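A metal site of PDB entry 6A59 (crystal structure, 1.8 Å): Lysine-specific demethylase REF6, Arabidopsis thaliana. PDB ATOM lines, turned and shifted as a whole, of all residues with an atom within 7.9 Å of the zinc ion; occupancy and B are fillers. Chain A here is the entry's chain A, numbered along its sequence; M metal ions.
The zinc ion is bound by SG of Cys 30 (2.2 Å), SG of Cys 25 (2.3 Å), NE2 of His 43 (2.4 Å) and NE2 of His 60 (2.6 Å).
The backbone NH (N) of Met 32 sits close to the side-chain sulfur (SG) of Cys 30 (3.6 Å).
N of Met 27 sits close to SG of Cys 25, 3.4 Å away.
O of Met 32 is in hydrogen-bond range of N of Cys 25 (3.0 Å).
N of His 60 lies close to ND2 of Asn 46 (3.3 Å).
Four residues have an atom within 4 Å of the zinc ion: Cys 25, Cys 30, His 43 and His 60.
Along chain A the residues within 4 Å of the zinc ion span positions 25 to 60.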
ATOM      1  N   GLN A  24      14.591 -12.558  21.277  1.00  0.00           N
ATOM      2  CA  GLN A  24      13.890 -13.850  21.224  1.00  0.00           C
ATOM      3  C   GLN A  24      14.827 -14.962  20.736  1.00  0.00           C
ATOM      4  O   GLN A  24      15.675 -14.714  19.869  1.00  0.00           O
ATOM      5  CB  GLN A  24      12.673 -13.764  20.295  1.00  0.00           C
ATOM      6  CG  GLN A  24      11.532 -12.887  20.801  1.00  0.00           C
ATOM      7  CD  GLN A  24      11.707 -11.391  20.552  1.00  0.00           C
ATOM      8  OE1 GLN A  24      12.497 -10.967  19.702  1.00  0.00           O
ATOM      9  NE2 GLN A  24      10.967 -10.579  21.313  1.00  0.00           N
ATOM     10  N   CYS A  25      14.690 -16.164  21.289  1.00  0.00           N
ATOM     11  CA  CYS A  25      15.434 -17.339  20.822  1.00  0.00           C
ATOM     12  C   CYS A  25      14.825 -17.876  19.527  1.00  0.00           C
ATOM     13  O   CYS A  25      13.597 -18.020  19.427  1.00  0.00           O
ATOM     14  CB  CYS A  25      15.453 -18.449  21.861  1.00  0.00           C
ATOM     15  SG  CYS A  25      16.355 -19.937  21.327  1.00  0.00           S
ATOM     16  N   ASN A  26      15.684 -18.206  18.562  1.00  0.00           N
ATOM     17  CA  ASN A  26      15.263 -18.700  17.243  1.00  0.00           C
ATOM     18  C   ASN A  26      15.299 -20.218  17.081  1.00  0.00           C
ATOM     19  O   ASN A  26      15.060 -20.722  15.979  1.00  0.00           O
ATOM     20  CB  ASN A  26      16.077 -18.018  16.124  1.00  0.00           C
ATOM     21  CG  ASN A  26      17.545 -18.429  16.104  1.00  0.00           C
ATOM     22  OD1 ASN A  26      18.071 -18.981  17.074  1.00  0.00           O
ATOM     23  ND2 ASN A  26      18.214 -18.156  14.987  1.00  0.00           N
ATOM     24  N   MET A  27      15.590 -20.957  18.159  1.00  0.00           N
ATOM     25  CA  MET A  27      15.580 -22.422  18.123  1.00  0.00           C
ATOM     26  C   MET A  27      14.157 -22.919  17.938  1.00  0.00           C
ATOM     27  O   MET A  27      13.213 -22.332  18.461  1.00  0.00           O
ATOM     28  CB  MET A  27      16.173 -23.011  19.404  1.00  0.00           C
ATOM     29  CG  MET A  27      17.670 -22.766  19.589  1.00  0.00           C
ATOM     30  SD  MET A  27      18.703 -23.781  18.507  1.00  0.00           S
ATOM     31  CE  MET A  27      19.111 -22.602  17.216  1.00  0.00           C
ATOM     32  N   GLU A  28      14.016 -24.011  17.179  1.00  0.00           N
ATOM     33  CA  GLU A  28      12.694 -24.552  16.844  1.00  0.00           C
ATOM     34  C   GLU A  28      11.930 -24.937  18.109  1.00  0.00           C
ATOM     35  O   GLU A  28      12.448 -25.679  18.951  1.00  0.00           O
ATOM     36  CB  GLU A  28      12.841 -25.766  15.904  1.00  0.00           C
ATOM     37  CG  GLU A  28      11.526 -26.346  15.372  1.00  0.00           C
ATOM     38  CD  GLU A  28      10.679 -25.335  14.620  1.00  0.00           C
ATOM     39  OE1 GLU A  28      11.236 -24.469  13.913  1.00  0.00           O
ATOM     40  OE2 GLU A  28       9.427 -25.405  14.731  1.00  0.00           O
ATOM     41  N   GLY A  29      10.732 -24.383  18.264  1.00  0.00           N
ATOM     42  CA  GLY A  29       9.880 -24.657  19.423  1.00  0.00           C
ATOM     43  C   GLY A  29      10.107 -23.780  20.649  1.00  0.00           C
ATOM     44  O   GLY A  29       9.275 -23.788  21.559  1.00  0.00           O
ATOM     45  N   CYS A  30      11.210 -23.024  20.694  1.00  0.00           N
ATOM     46  CA  CYS A  30      11.541 -22.234  21.875  1.00  0.00           C
ATOM     47  C   CYS A  30      10.719 -20.950  21.935  1.00  0.00           C
ATOM     48  O   CYS A  30      10.528 -20.279  20.916  1.00  0.00           O
ATOM     49  CB  CYS A  30      13.028 -21.860  21.907  1.00  0.00           C
ATOM     50  SG  CYS A  30      13.559 -21.281  23.531  1.00  0.00           S
ATOM     51  N   THR A  31      10.235 -20.623  23.129  1.00  0.00           N
ATOM     52  CA  THR A  31       9.434 -19.425  23.350  1.00  0.00           C
ATOM     53  C   THR A  31      10.099 -18.457  24.343  1.00  0.00           C
ATOM     54  O   THR A  31       9.446 -17.526  24.822  1.00  0.00           O
ATOM     55  CB  THR A  31       8.014 -19.789  23.829  1.00  0.00           C
ATOM     56  OG1 THR A  31       8.100 -20.496  25.076  1.00  0.00           O
ATOM     57  CG2 THR A  31       7.308 -20.658  22.790  1.00  0.00           C
ATOM     58  N   MET A  32      11.382 -18.661  24.628  1.00  0.00           N
ATOM     59  CA  MET A  32      12.096 -17.825  25.588  1.00  0.00           C
ATOM     60  C   MET A  32      12.612 -16.538  24.954  1.00  0.00           C
ATOM     61  O   MET A  32      12.920 -16.510  23.747  1.00  0.00           O
ATOM     62  CB  MET A  32      13.256 -18.583  26.224  1.00  0.00           C
ATOM     63  CG  MET A  32      12.808 -19.826  26.960  1.00  0.00           C
ATOM     64  SD  MET A  32      14.117 -20.554  27.946  1.00  0.00           S
ATOM     65  CE  MET A  32      13.493 -22.215  28.137  1.00  0.00           C
ATOM     66  N   SER A  33      12.689 -15.491  25.766  1.00  0.00           N
ATOM     67  CA  SER A  33      13.255 -14.198  25.362  1.00  0.00           C
ATOM     68  C   SER A  33      14.131 -13.663  26.492  1.00  0.00           C
ATOM     69  O   SER A  33      14.021 -14.100  27.628  1.00  0.00           O
ATOM     70  CB  SER A  33      12.142 -13.209  25.033  1.00  0.00           C
ATOM     71  OG  SER A  33      11.343 -12.943  26.161  1.00  0.00           O
ATOM     72  N   PHE A  34      14.998 -12.706  26.142  1.00  0.00           N
ATOM     73  CA  PHE A  34      16.075 -12.252  27.017  1.00  0.00           C
ATOM     74  C   PHE A  34      16.273 -10.736  26.958  1.00  0.00           C
ATOM     75  O   PHE A  34      15.950 -10.106  25.951  1.00  0.00           O
ATOM     76  CB  PHE A  34      17.377 -12.991  26.661  1.00  0.00           C
ATOM     77  CG  PHE A  34      17.259 -14.469  26.816  1.00  0.00           C
ATOM     78  CD1 PHE A  34      17.450 -15.052  28.062  1.00  0.00           C
ATOM     79  CD2 PHE A  34      16.866 -15.270  25.749  1.00  0.00           C
ATOM     80  CE1 PHE A  34      17.299 -16.404  28.237  1.00  0.00           C
ATOM     81  CE2 PHE A  34      16.704 -16.637  25.918  1.00  0.00           C
ATOM     82  CZ  PHE A  34      16.924 -17.204  27.169  1.00  0.00           C
ATOM     83  N   LEU A  40      21.076 -14.011  25.521  1.00  0.00           N
ATOM     84  CA  LEU A  40      20.661 -14.847  24.369  1.00  0.00           C
ATOM     85  C   LEU A  40      21.800 -15.739  23.895  1.00  0.00           C
ATOM     86  O   LEU A  40      21.587 -16.910  23.582  1.00  0.00           O
ATOM     87  CB  LEU A  40      20.152 -13.973  23.209  1.00  0.00           C
ATOM     88  CG  LEU A  40      19.753 -14.693  21.919  1.00  0.00           C
ATOM     89  CD1 LEU A  40      18.633 -15.701  22.170  1.00  0.00           C
ATOM     90  CD2 LEU A  40      19.342 -13.703  20.835  1.00  0.00           C
ATOM     91  N   HIS A  43      22.253 -18.436  26.386  1.00  0.00           N
ATOM     92  CA  HIS A  43      21.143 -19.367  26.130  1.00  0.00           C
ATOM     93  C   HIS A  43      21.422 -20.324  24.976  1.00  0.00           C
ATOM     94  O   HIS A  43      21.156 -21.518  25.075  1.00  0.00           O
ATOM     95  CB  HIS A  43      19.861 -18.597  25.843  1.00  0.00           C
ATOM     96  CG  HIS A  43      18.658 -19.476  25.709  1.00  0.00           C
ATOM     97  ND1 HIS A  43      18.236 -20.284  26.735  1.00  0.00           N
ATOM     98  CD2 HIS A  43      17.794 -19.665  24.692  1.00  0.00           C
ATOM     99  CE1 HIS A  43      17.153 -20.935  26.353  1.00  0.00           C
ATOM    100  NE2 HIS A  43      16.867 -20.583  25.112  1.00  0.00           N
ATOM    101  N   LYS A  44      21.978 -19.794  23.881  1.00  0.00           N
ATOM    102  CA  LYS A  44      22.380 -20.613  22.725  1.00  0.00           C
ATOM    103  C   LYS A  44      23.516 -21.621  23.032  1.00  0.00           C
ATOM    104  O   LYS A  44      23.643 -22.633  22.345  1.00  0.00           O
ATOM    105  CB  LYS A  44      22.736 -19.734  21.532  1.00  0.00           C
ATOM    106  CG  LYS A  44      21.539 -19.070  20.894  1.00  0.00           C
ATOM    107  CD  LYS A  44      21.952 -18.050  19.847  1.00  0.00           C
ATOM    108  CE  LYS A  44      20.845 -17.789  18.839  1.00  0.00           C
ATOM    109  NZ  LYS A  44      20.616 -18.953  17.929  1.00  0.00           N
ATOM    110  N   ASN A  46      23.362 -23.290  25.692  1.00  0.00           N
ATOM    111  CA  ASN A  46      22.633 -24.199  26.585  1.00  0.00           C
ATOM    112  C   ASN A  46      22.986 -24.057  28.073  1.00  0.00           C
ATOM    113  O   ASN A  46      23.050 -25.055  28.803  1.00  0.00           O
ATOM    114  CB  ASN A  46      22.768 -25.660  26.111  1.00  0.00           C
ATOM    115  CG  ASN A  46      22.311 -25.856  24.674  1.00  0.00           C
ATOM    116  OD1 ASN A  46      22.990 -26.507  23.882  1.00  0.00           O
ATOM    117  ND2 ASN A  46      21.150 -25.322  24.335  1.00  0.00           N
ATOM    118  N   HIS A  60      19.520 -28.062  23.473  1.00  0.00           N
ATOM    119  CA  HIS A  60      18.449 -27.137  23.836  1.00  0.00           C
ATOM    120  C   HIS A  60      17.249 -27.870  24.448  1.00  0.00           C
ATOM    121  O   HIS A  60      16.597 -27.319  25.336  1.00  0.00           O
ATOM    122  CB  HIS A  60      18.047 -26.295  22.624  1.00  0.00           C
ATOM    123  CG  HIS A  60      16.888 -25.386  22.886  1.00  0.00           C
ATOM    124  ND1 HIS A  60      15.602 -25.699  22.510  1.00  0.00           N
ATOM    125  CD2 HIS A  60      16.824 -24.180  23.501  1.00  0.00           C
ATOM    126  CE1 HIS A  60      14.790 -24.736  22.881  1.00  0.00           C
ATOM    127  NE2 HIS A  60      15.505 -23.797  23.482  1.00  0.00           N
ATOM    128  N   LEU A  63      18.045 -28.355  28.073  1.00  0.00           N
ATOM    129  CA  LEU A  63      17.969 -27.050  28.730  1.00  0.00           C
ATOM    130  C   LEU A  63      16.532 -26.685  29.107  1.00  0.00           C
ATOM    131  O   LEU A  63      16.277 -26.256  30.234  1.00  0.00           O
ATOM    132  CB  LEU A  63      18.556 -25.969  27.827  1.00  0.00           C
ATOM    133  CG  LEU A  63      18.566 -24.539  28.378  1.00  0.00           C
ATOM    134  CD1 LEU A  63      19.580 -24.417  29.506  1.00  0.00           C
ATOM    135  CD2 LEU A  63      18.867 -23.572  27.259  1.00  0.00           C
ATOM    136  N   VAL A  64      15.611 -26.820  28.152  1.00  0.00           N
ATOM    137  CA  VAL A  64      14.203 -26.444  28.360  1.00  0.00           C
ATOM    138  C   VAL A  64      13.549 -27.346  29.417  1.00  0.00           C
ATOM    139  O   VAL A  64      12.800 -26.855  30.278  1.00  0.00           O
ATOM    140  CB  VAL A  64      13.388 -26.486  27.039  1.00  0.00           C
ATOM    141  CG1 VAL A  64      11.896 -26.290  27.271  1.00  0.00           C
ATOM    142  CG2 VAL A  64      13.910 -25.420  26.083  1.00  0.00           C
HETATM  143 ZN    ZN M   1      15.760 -21.236  23.132  1.00  0.00          ZN
